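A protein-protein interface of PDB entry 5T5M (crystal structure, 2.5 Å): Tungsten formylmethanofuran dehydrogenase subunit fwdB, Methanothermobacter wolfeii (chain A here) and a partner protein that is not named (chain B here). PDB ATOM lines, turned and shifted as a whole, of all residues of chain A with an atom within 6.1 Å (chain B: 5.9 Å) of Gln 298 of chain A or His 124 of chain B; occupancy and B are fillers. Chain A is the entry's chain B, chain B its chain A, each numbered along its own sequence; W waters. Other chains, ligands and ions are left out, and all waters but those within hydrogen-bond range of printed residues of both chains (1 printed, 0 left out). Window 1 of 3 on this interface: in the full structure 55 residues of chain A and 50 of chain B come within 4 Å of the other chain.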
ATOM      1  N   CYS A  94      35.574  -7.525  21.420  1.00  0.00           N
ATOM      2  CA  CYS A  94      34.671  -7.867  22.510  1.00  0.00           C
ATOM      3  C   CYS A  94      34.724  -9.346  22.878  1.00  0.00           C
ATOM      4  O   CYS A  94      34.468  -9.696  24.032  1.00  0.00           O
ATOM      5  CB  CYS A  94      33.242  -7.463  22.142  1.00  0.00           C
ATOM      6  SG  CYS A  94      32.908  -5.688  22.258  1.00  0.00           S
ATOM      7  N   VAL A 293      36.837   0.996  24.345  1.00  0.00           N
ATOM      8  CA  VAL A 293      36.605   1.066  25.789  1.00  0.00           C
ATOM      9  C   VAL A 293      35.124   0.844  26.086  1.00  0.00           C
ATOM     10  O   VAL A 293      34.763   0.131  27.030  1.00  0.00           O
ATOM     11  CB  VAL A 293      37.113   2.399  26.371  1.00  0.00           C
ATOM     12  CG1 VAL A 293      36.391   3.599  25.752  1.00  0.00           C
ATOM     13  CG2 VAL A 293      36.960   2.415  27.903  1.00  0.00           C
ATOM     14  N   THR A 294      34.245   1.427  25.264  1.00  0.00           N
ATOM     15  CA  THR A 294      32.810   1.229  25.434  1.00  0.00           C
ATOM     16  C   THR A 294      32.435  -0.243  25.337  1.00  0.00           C
ATOM     17  O   THR A 294      31.528  -0.710  26.032  1.00  0.00           O
ATOM     18  CB  THR A 294      32.068   2.029  24.376  1.00  0.00           C
ATOM     19  OG1 THR A 294      32.527   3.384  24.410  1.00  0.00           O
ATOM     20  CG2 THR A 294      30.555   1.969  24.607  1.00  0.00           C
ATOM     21  N   GLY A 295      33.118  -0.987  24.472  1.00  0.00           N
ATOM     22  CA  GLY A 295      32.806  -2.396  24.317  1.00  0.00           C
ATOM     23  C   GLY A 295      33.063  -3.209  25.570  1.00  0.00           C
ATOM     24  O   GLY A 295      32.284  -4.105  25.902  1.00  0.00           O
ATOM     25  N   PHE A 296      34.168  -2.939  26.277  1.00  0.00           N
ATOM     26  CA  PHE A 296      34.414  -3.718  27.489  1.00  0.00           C
ATOM     27  C   PHE A 296      33.334  -3.459  28.523  1.00  0.00           C
ATOM     28  O   PHE A 296      32.871  -4.390  29.189  1.00  0.00           O
ATOM     29  CB  PHE A 296      35.779  -3.424  28.103  1.00  0.00           C
ATOM     30  CG  PHE A 296      35.996  -4.135  29.424  1.00  0.00           C
ATOM     31  CD1 PHE A 296      36.502  -5.424  29.458  1.00  0.00           C
ATOM     32  CD2 PHE A 296      35.643  -3.537  30.622  1.00  0.00           C
ATOM     33  CE1 PHE A 296      36.678  -6.084  30.664  1.00  0.00           C
ATOM     34  CE2 PHE A 296      35.822  -4.192  31.823  1.00  0.00           C
ATOM     35  CZ  PHE A 296      36.339  -5.466  31.843  1.00  0.00           C
ATOM     36  N   ASN A 297      32.921  -2.201  28.676  1.00  0.00           N
ATOM     37  CA  ASN A 297      31.889  -1.905  29.658  1.00  0.00           C
ATOM     38  C   ASN A 297      30.570  -2.551  29.271  1.00  0.00           C
ATOM     39  O   ASN A 297      29.835  -3.012  30.149  1.00  0.00           O
ATOM     40  CB  ASN A 297      31.728  -0.394  29.831  1.00  0.00           C
ATOM     41  CG  ASN A 297      33.013   0.272  30.273  1.00  0.00           C
ATOM     42  OD1 ASN A 297      33.413   1.299  29.720  1.00  0.00           O
ATOM     43  ND2 ASN A 297      33.680  -0.318  31.268  1.00  0.00           N
ATOM     44  N   GLN A 298      30.267  -2.627  27.970  1.00  0.00           N
ATOM     45  CA  GLN A 298      29.071  -3.341  27.538  1.00  0.00           C
ATOM     46  C   GLN A 298      29.158  -4.807  27.940  1.00  0.00           C
ATOM     47  O   GLN A 298      28.289  -5.320  28.655  1.00  0.00           O
ATOM     48  CB  GLN A 298      28.874  -3.196  26.022  1.00  0.00           C
ATOM     49  CG  GLN A 298      28.643  -1.757  25.548  1.00  0.00           C
ATOM     50  CD  GLN A 298      27.225  -1.286  25.759  1.00  0.00           C
ATOM     51  OE1 GLN A 298      26.401  -1.985  26.347  1.00  0.00           O
ATOM     52  NE2 GLN A 298      26.928  -0.092  25.273  1.00  0.00           N
ATOM     53  N   VAL A 299      30.239  -5.483  27.529  1.00  0.00           N
ATOM     54  CA  VAL A 299      30.379  -6.920  27.757  1.00  0.00           C
ATOM     55  C   VAL A 299      30.313  -7.236  29.243  1.00  0.00           C
ATOM     56  O   VAL A 299      29.562  -8.116  29.679  1.00  0.00           O
ATOM     57  CB  VAL A 299      31.703  -7.429  27.154  1.00  0.00           C
ATOM     58  CG1 VAL A 299      31.999  -8.835  27.639  1.00  0.00           C
ATOM     59  CG2 VAL A 299      31.668  -7.375  25.628  1.00  0.00           C
ATOM     60  N   CYS A 300      31.150  -6.559  30.030  1.00  0.00           N
ATOM     61  CA  CYS A 300      31.220  -6.812  31.462  1.00  0.00           C
ATOM     62  C   CYS A 300      29.857  -6.621  32.116  1.00  0.00           C
ATOM     63  O   CYS A 300      29.430  -7.447  32.932  1.00  0.00           O
ATOM     64  CB  CYS A 300      32.271  -5.885  32.081  1.00  0.00           C
ATOM     65  SG  CYS A 300      32.860  -6.356  33.719  1.00  0.00           S
ATOM     66  N   THR A 301      29.138  -5.559  31.732  1.00  0.00           N
ATOM     67  CA  THR A 301      27.835  -5.289  32.327  1.00  0.00           C
ATOM     68  C   THR A 301      26.855  -6.418  32.053  1.00  0.00           C
ATOM     69  O   THR A 301      26.161  -6.883  32.965  1.00  0.00           O
ATOM     70  CB  THR A 301      27.272  -3.972  31.798  1.00  0.00           C
ATOM     71  OG1 THR A 301      28.178  -2.910  32.107  1.00  0.00           O
ATOM     72  CG2 THR A 301      25.912  -3.681  32.430  1.00  0.00           C
ATOM     73  N   TRP A 302      26.771  -6.872  30.795  1.00  0.00           N
ATOM     74  CA  TRP A 302      25.751  -7.858  30.449  1.00  0.00           C
ATOM     75  C   TRP A 302      26.092  -9.252  30.947  1.00  0.00           C
ATOM     76  O   TRP A 302      25.181 -10.065  31.129  1.00  0.00           O
ATOM     77  CB  TRP A 302      25.473  -7.860  28.925  1.00  0.00           C
ATOM     78  CG  TRP A 302      26.390  -8.635  27.971  1.00  0.00           C
ATOM     79  CD1 TRP A 302      26.762  -9.951  28.045  1.00  0.00           C
ATOM     80  CD2 TRP A 302      26.966  -8.129  26.759  1.00  0.00           C
ATOM     81  NE1 TRP A 302      27.541 -10.285  26.962  1.00  0.00           N
ATOM     82  CE2 TRP A 302      27.679  -9.186  26.156  1.00  0.00           C
ATOM     83  CE3 TRP A 302      26.938  -6.882  26.119  1.00  0.00           C
ATOM     84  CZ2 TRP A 302      28.376  -9.029  24.954  1.00  0.00           C
ATOM     85  CZ3 TRP A 302      27.628  -6.732  24.916  1.00  0.00           C
ATOM     86  CH2 TRP A 302      28.332  -7.798  24.349  1.00  0.00           C
ATOM     87  N   GLU A 303      27.365  -9.533  31.215  1.00  0.00           N
ATOM     88  CA  GLU A 303      27.751 -10.838  31.735  1.00  0.00           C
ATOM     89  C   GLU A 303      27.670 -10.902  33.256  1.00  0.00           C
ATOM     90  O   GLU A 303      27.200 -11.903  33.807  1.00  0.00           O
ATOM     91  CB  GLU A 303      29.172 -11.184  31.288  1.00  0.00           C
ATOM     92  CG  GLU A 303      29.315 -11.532  29.807  1.00  0.00           C
ATOM     93  CD  GLU A 303      30.504 -12.450  29.547  1.00  0.00           C
ATOM     94  OE1 GLU A 303      31.287 -12.687  30.491  1.00  0.00           O
ATOM     95  OE2 GLU A 303      30.649 -12.946  28.412  1.00  0.00           O
ATOM     96  N   PRO A 307      29.732  -2.708  35.283  1.00  0.00           N
ATOM     97  CA  PRO A 307      30.475  -2.251  34.092  1.00  0.00           C
ATOM     98  C   PRO A 307      32.001  -2.280  34.169  1.00  0.00           C
ATOM     99  O   PRO A 307      32.654  -2.427  33.130  1.00  0.00           O
ATOM    100  CB  PRO A 307      29.989  -0.808  33.930  1.00  0.00           C
ATOM    101  CG  PRO A 307      29.648  -0.380  35.326  1.00  0.00           C
ATOM    102  CD  PRO A 307      29.120  -1.590  36.020  1.00  0.00           C
ATOM    103  N   TYR A 394      32.601  -1.106  20.045  1.00  0.00           N
ATOM    104  CA  TYR A 394      31.478  -0.212  20.316  1.00  0.00           C
ATOM    105  C   TYR A 394      31.941   1.234  20.260  1.00  0.00           C
ATOM    106  O   TYR A 394      32.818   1.648  21.029  1.00  0.00           O
ATOM    107  CB  TYR A 394      30.831  -0.512  21.672  1.00  0.00           C
ATOM    108  CG  TYR A 394      29.938  -1.721  21.630  1.00  0.00           C
ATOM    109  CD1 TYR A 394      30.471  -2.992  21.465  1.00  0.00           C
ATOM    110  CD2 TYR A 394      28.565  -1.594  21.736  1.00  0.00           C
ATOM    111  CE1 TYR A 394      29.660  -4.105  21.414  1.00  0.00           C
ATOM    112  CE2 TYR A 394      27.745  -2.704  21.688  1.00  0.00           C
ATOM    113  CZ  TYR A 394      28.300  -3.954  21.528  1.00  0.00           C
ATOM    114  OH  TYR A 394      27.500  -5.061  21.480  1.00  0.00           O
ATOM    115  N   GLY A 398      27.587   3.753  21.704  1.00  0.00           N
ATOM    116  CA  GLY A 398      27.014   2.427  21.830  1.00  0.00           C
ATOM    117  C   GLY A 398      26.770   1.683  20.541  1.00  0.00           C
ATOM    118  O   GLY A 398      26.186   0.594  20.581  1.00  0.00           O
ATOM    119  N   PRO A 400      27.516  -0.794  17.751  1.00  0.00           N
ATOM    120  CA  PRO A 400      28.450  -1.912  17.548  1.00  0.00           C
ATOM    121  C   PRO A 400      28.868  -1.993  16.085  1.00  0.00           C
ATOM    122  O   PRO A 400      28.020  -2.081  15.193  1.00  0.00           O
ATOM    123  CB  PRO A 400      27.623  -3.135  17.965  1.00  0.00           C
ATOM    124  CG  PRO A 400      26.209  -2.759  17.576  1.00  0.00           C
ATOM    125  CD  PRO A 400      26.113  -1.256  17.809  1.00  0.00           C
ATOM    126  N   ALA B  61      17.715  -8.675  25.890  1.00  0.00           N
ATOM    127  CA  ALA B  61      18.951  -8.624  25.109  1.00  0.00           C
ATOM    128  C   ALA B  61      19.010  -7.336  24.305  1.00  0.00           C
ATOM    129  O   ALA B  61      18.140  -7.091  23.463  1.00  0.00           O
ATOM    130  CB  ALA B  61      19.052  -9.833  24.172  1.00  0.00           C
ATOM    131  N   GLY B  62      20.038  -6.522  24.548  1.00  0.00           N
ATOM    132  CA  GLY B  62      20.295  -5.378  23.706  1.00  0.00           C
ATOM    133  C   GLY B  62      20.574  -4.119  24.499  1.00  0.00           C
ATOM    134  O   GLY B  62      20.760  -4.143  25.719  1.00  0.00           O
ATOM    135  N   ALA B  63      20.571  -2.997  23.775  1.00  0.00           N
ATOM    136  CA  ALA B  63      21.125  -1.745  24.279  1.00  0.00           C
ATOM    137  C   ALA B  63      20.333  -1.210  25.471  1.00  0.00           C
ATOM    138  O   ALA B  63      20.914  -0.891  26.512  1.00  0.00           O
ATOM    139  CB  ALA B  63      21.165  -0.714  23.149  1.00  0.00           C
ATOM    140  N   ASN B  66      20.853  -3.240  28.553  1.00  0.00           N
ATOM    141  CA  ASN B  66      22.161  -3.170  29.190  1.00  0.00           C
ATOM    142  C   ASN B  66      22.392  -1.827  29.866  1.00  0.00           C
ATOM    143  O   ASN B  66      23.180  -1.752  30.812  1.00  0.00           O
ATOM    144  CB  ASN B  66      23.269  -3.447  28.177  1.00  0.00           C
ATOM    145  CG  ASN B  66      24.463  -4.143  28.796  1.00  0.00           C
ATOM    146  OD1 ASN B  66      24.330  -4.952  29.726  1.00  0.00           O
ATOM    147  ND2 ASN B  66      25.642  -3.832  28.283  1.00  0.00           N
ATOM    148  N   VAL B  67      21.728  -0.767  29.401  1.00  0.00           N
ATOM    149  CA  VAL B  67      21.762   0.502  30.120  1.00  0.00           C
ATOM    150  C   VAL B  67      21.121   0.336  31.490  1.00  0.00           C
ATOM    151  O   VAL B  67      21.661   0.789  32.505  1.00  0.00           O
ATOM    152  CB  VAL B  67      21.068   1.608  29.307  1.00  0.00           C
ATOM    153  CG1 VAL B  67      20.986   2.894  30.122  1.00  0.00           C
ATOM    154  CG2 VAL B  67      21.818   1.872  28.033  1.00  0.00           C
ATOM    155  N   ARG B  69      20.901  -2.432  33.146  1.00  0.00           N
ATOM    156  CA  ARG B  69      21.880  -3.190  33.915  1.00  0.00           C
ATOM    157  C   ARG B  69      22.985  -2.274  34.431  1.00  0.00           C
ATOM    158  O   ARG B  69      23.352  -2.322  35.614  1.00  0.00           O
ATOM    159  CB  ARG B  69      22.486  -4.311  33.066  1.00  0.00           C
ATOM    160  CG  ARG B  69      21.534  -5.424  32.616  1.00  0.00           C
ATOM    161  CD  ARG B  69      22.344  -6.598  32.060  1.00  0.00           C
ATOM    162  NE  ARG B  69      21.527  -7.597  31.369  1.00  0.00           N
ATOM    163  CZ  ARG B  69      21.374  -7.661  30.050  1.00  0.00           C
ATOM    164  NH1 ARG B  69      21.982  -6.788  29.254  1.00  0.00           N
ATOM    165  NH2 ARG B  69      20.610  -8.608  29.516  1.00  0.00           N
ATOM    166  N   MET B  70      23.525  -1.427  33.552  1.00  0.00           N
ATOM    167  CA  MET B  70      24.704  -0.652  33.913  1.00  0.00           C
ATOM    168  C   MET B  70      24.371   0.413  34.953  1.00  0.00           C
ATOM    169  O   MET B  70      25.079   0.564  35.959  1.00  0.00           O
ATOM    170  CB  MET B  70      25.307  -0.004  32.673  1.00  0.00           C
ATOM    171  CG  MET B  70      26.628   0.687  32.958  1.00  0.00           C
ATOM    172  SD  MET B  70      27.314   1.623  31.573  1.00  0.00           S
ATOM    173  CE  MET B  70      27.728   0.336  30.401  1.00  0.00           C
ATOM    174  N   LEU B 121      21.534  -1.350  16.158  1.00  0.00           N
ATOM    175  CA  LEU B 121      22.143  -1.940  17.345  1.00  0.00           C
ATOM    176  C   LEU B 121      21.928  -3.449  17.409  1.00  0.00           C
ATOM    177  O   LEU B 121      22.023  -4.042  18.490  1.00  0.00           O
ATOM    178  CB  LEU B 121      21.589  -1.264  18.601  1.00  0.00           C
ATOM    179  CG  LEU B 121      21.587   0.266  18.548  1.00  0.00           C
ATOM    180  CD1 LEU B 121      20.986   0.881  19.841  1.00  0.00           C
ATOM    181  CD2 LEU B 121      22.988   0.815  18.298  1.00  0.00           C
ATOM    182  N   ALA B 122      21.661  -4.083  16.261  1.00  0.00           N
ATOM    183  CA  ALA B 122      21.305  -5.497  16.247  1.00  0.00           C
ATOM    184  C   ALA B 122      22.456  -6.384  16.706  1.00  0.00           C
ATOM    185  O   ALA B 122      22.222  -7.408  17.361  1.00  0.00           O
ATOM    186  CB  ALA B 122      20.842  -5.899  14.845  1.00  0.00           C
ATOM    187  N   ARG B 123      23.700  -6.022  16.374  1.00  0.00           N
ATOM    188  CA  ARG B 123      24.826  -6.839  16.809  1.00  0.00           C
ATOM    189  C   ARG B 123      24.856  -6.975  18.321  1.00  0.00           C
ATOM    190  O   ARG B 123      25.232  -8.035  18.840  1.00  0.00           O
ATOM    191  CB  ARG B 123      26.137  -6.244  16.309  1.00  0.00           C
ATOM    192  CG  ARG B 123      26.660  -6.883  15.032  1.00  0.00           C
ATOM    193  CD  ARG B 123      27.879  -6.140  14.522  1.00  0.00           C
ATOM    194  NE  ARG B 123      27.519  -4.815  14.030  1.00  0.00           N
ATOM    195  CZ  ARG B 123      27.095  -4.561  12.794  1.00  0.00           C
ATOM    196  NH1 ARG B 123      26.778  -3.318  12.451  1.00  0.00           N
ATOM    197  NH2 ARG B 123      26.987  -5.542  11.893  1.00  0.00           N
ATOM    198  N   HIS B 124      24.454  -5.917  19.037  1.00  0.00           N
ATOM    199  CA  HIS B 124      24.469  -5.926  20.495  1.00  0.00           C
ATOM    200  C   HIS B 124      23.468  -6.934  21.049  1.00  0.00           C
ATOM    201  O   HIS B 124      23.779  -7.687  21.980  1.00  0.00           O
ATOM    202  CB  HIS B 124      24.167  -4.515  21.004  1.00  0.00           C
ATOM    203  CG  HIS B 124      24.274  -4.354  22.490  1.00  0.00           C
ATOM    204  ND1 HIS B 124      24.412  -3.118  23.083  1.00  0.00           N
ATOM    205  CD2 HIS B 124      24.242  -5.257  23.500  1.00  0.00           C
ATOM    206  CE1 HIS B 124      24.473  -3.267  24.393  1.00  0.00           C
ATOM    207  NE2 HIS B 124      24.365  -4.555  24.673  1.00  0.00           N
ATOM    208  N   THR B 125      22.255  -6.952  20.497  1.00  0.00           N
ATOM    209  CA  THR B 125      21.253  -7.926  20.918  1.00  0.00           C
ATOM    210  C   THR B 125      21.768  -9.350  20.751  1.00  0.00           C
ATOM    211  O   THR B 125      21.680 -10.167  21.676  1.00  0.00           O
ATOM    212  CB  THR B 125      19.965  -7.728  20.115  1.00  0.00           C
ATOM    213  OG1 THR B 125      19.366  -6.477  20.463  1.00  0.00           O
ATOM    214  CG2 THR B 125      18.960  -8.865  20.368  1.00  0.00           C
ATOM    215  N   HIS B 126      22.309  -9.669  19.572  1.00  0.00           N
ATOM    216  CA  HIS B 126      22.732 -11.042  19.305  1.00  0.00           C
ATOM    217  C   HIS B 126      23.911 -11.444  20.180  1.00  0.00           C
ATOM    218  O   HIS B 126      24.012 -12.603  20.599  1.00  0.00           O
ATOM    219  CB  HIS B 126      23.080 -11.214  17.825  1.00  0.00           C
ATOM    220  CG  HIS B 126      21.891 -11.140  16.924  1.00  0.00           C
ATOM    221  ND1 HIS B 126      20.892 -12.092  16.935  1.00  0.00           N
ATOM    222  CD2 HIS B 126      21.525 -10.217  16.002  1.00  0.00           C
ATOM    223  CE1 HIS B 126      19.966 -11.761  16.053  1.00  0.00           C
ATOM    224  NE2 HIS B 126      20.325 -10.629  15.473  1.00  0.00           N
ATOM    225  N   GLU B 127      24.815 -10.511  20.468  1.00  0.00           N
ATOM    226  CA  GLU B 127      25.941 -10.834  21.335  1.00  0.00           C
ATOM    227  C   GLU B 127      25.473 -11.207  22.740  1.00  0.00           C
ATOM    228  O   GLU B 127      25.997 -12.152  23.342  1.00  0.00           O
ATOM    229  CB  GLU B 127      26.923  -9.663  21.367  1.00  0.00           C
ATOM    230  CG  GLU B 127      27.840  -9.631  20.159  1.00  0.00           C
ATOM    231  CD  GLU B 127      28.972  -8.636  20.299  1.00  0.00           C
ATOM    232  OE1 GLU B 127      28.710  -7.498  20.733  1.00  0.00           O
ATOM    233  OE2 GLU B 127      30.128  -9.000  19.974  1.00  0.00           O
ATOM    234  N   GLU B 128      24.492 -10.482  23.286  1.00  0.00           N
ATOM    235  CA  GLU B 128      23.959 -10.870  24.589  1.00  0.00           C
ATOM    236  C   GLU B 128      23.235 -12.209  24.498  1.00  0.00           C
ATOM    237  O   GLU B 128      23.352 -13.048  25.398  1.00  0.00           O
ATOM    238  CB  GLU B 128      23.028  -9.785  25.141  1.00  0.00           C
ATOM    239  CG  GLU B 128      23.694  -8.447  25.408  1.00  0.00           C
ATOM    240  CD  GLU B 128      22.839  -7.499  26.278  1.00  0.00           C
ATOM    241  OE1 GLU B 128      21.760  -7.914  26.769  1.00  0.00           O
ATOM    242  OE2 GLU B 128      23.248  -6.329  26.468  1.00  0.00           O
ATOM    243  N   PHE B 129      22.488 -12.434  23.414  1.00  0.00           N
ATOM    244  CA  PHE B 129      21.861 -13.735  23.224  1.00  0.00           C
ATOM    245  C   PHE B 129      22.880 -14.860  23.331  1.00  0.00           C
ATOM    246  O   PHE B 129      22.631 -15.872  23.994  1.00  0.00           O
ATOM    247  CB  PHE B 129      21.160 -13.785  21.862  1.00  0.00           C
ATOM    248  CG  PHE B 129      19.730 -13.306  21.881  1.00  0.00           C
ATOM    249  CD1 PHE B 129      18.920 -13.517  22.987  1.00  0.00           C
ATOM    250  CD2 PHE B 129      19.194 -12.651  20.776  1.00  0.00           C
ATOM    251  CE1 PHE B 129      17.609 -13.083  22.998  1.00  0.00           C
ATOM    252  CE2 PHE B 129      17.876 -12.209  20.783  1.00  0.00           C
ATOM    253  CZ  PHE B 129      17.086 -12.429  21.899  1.00  0.00           C
HETATM  254  O   HOH W   1      25.941  -1.182  13.897  1.00  0.00           O
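The side-chain amide oxygen (OE1) of Gln 298 of chain A lies within hydrogen-bond range of the side-chain amide nitrogen (ND2) of Asn 66 of chain B (2.8 Å).
The backbone NH (N) of Trp 302 of chain A lies close to the side-chain amide oxygen (OD1) of Asn 66 of chain B.
The backbone carbonyl oxygen (O) of Pro 400 of chain A is in hydrogen-bond range of the guanidinium group (NE) of Arg 123 of chain B.
OH of Tyr 394 of chain A sits at hydrogen-bond distance from OE1 of Glu 127 of chain B (2.8 Å).
The backbone NH (N) of Gly 62 of chain B is in hydrogen-bond range of the side-chain carboxylate (OE1) of Glu 128 of chain B (3.1 Å).
The side-chain amide oxygen (OD1) of Asn 66 of chain B is in hydrogen-bond range of the guanidinium group (NH1) of Arg 69 of chain B, 3.0 Å away.
NH1 of Arg 69 of chain B lies within salt-bridge range of OE1 of Glu 128 of chain B (2.7 Å).
OE2 of Glu 128 of chain B lies within hydrogen-bond range of NE2 of His 124 of chain B (2.8 Å).
The backbone carbonyl oxygen of Val 293 of chain A sits close to the side-chain amide oxygen of Asn 297 of chain A (3.2 Å).
The backbone carbonyl oxygen (O) of Pro 307 of chain A lies within hydrogen-bond range of the side-chain amide nitrogen (ND2) of Asn 297 of chain A, at 3.0 Å.
Met 70 of chain B touches Asn 297 of chain A (CE to O, 3.96 Å).
OE1 of Gln 298 of chain A touches CE1 of His 124 of chain B, at 3.0 Å.
Thr 301 of chain A touches Arg 69 of chain B (CG2 to CB, 3.5 Å).
Thr 301 of chain A touches Met 70 of chain B (CG2 to N, 3.5 Å).
Trp 302 of chain A touches Arg 69 of chain B.
CE3 of Trp 302 of chain A touches NE2 of His 124 of chain B (3.8 Å).
Trp 302 of chain A touches Glu 127 of chain B (CH2 to OE1, 3.6 Å).
Trp 302 of chain A touches Glu 128 of chain B.
Leu 121 of chain B touches Gly 398 of chain A (CD2 to O, 3.9 Å).
CG of Pro 400 of chain A touches N of His 124 of chain B (3.9 Å).
Of chain B, only Asn 66 and His 124 come within 4 Å of Gln 298 of chain A.
Printed residues of chain B within 4 Å of Gly 398 of chain A: Leu 121 (3.9 Å).
Of the printed residues of chain A, Met 70 of chain B touches Asn 297 (3.96 Å), Thr 301 (3.5 Å) and Pro 307 (3.8 Å).
Of the printed residues of chain A, His 124 of chain B touches Gln 298, Trp 302, Tyr 394 and Pro 400.
The nearest printed residue of chain B that does not touch Thr 301 of chain A is Val 67 of chain B (5.9 Å).
Hydrophobic or aromatic side chains of chain B within 4 Å of the printed part of chain A: Met 70, Leu 121 and His 124.
Hydrophobic or aromatic side chains of chain A within 4 Å of the printed part of chain B: Trp 302, Pro 307, Tyr 394 and Pro 400.
Among the printed residues, 18 pairs touch across the chains.
Water W1 bridges the backbone carbonyl oxygen of Pro 400 of chain A (2.6 Å) and the guanidinium group of Arg 123 of chain B (2.7 Å).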
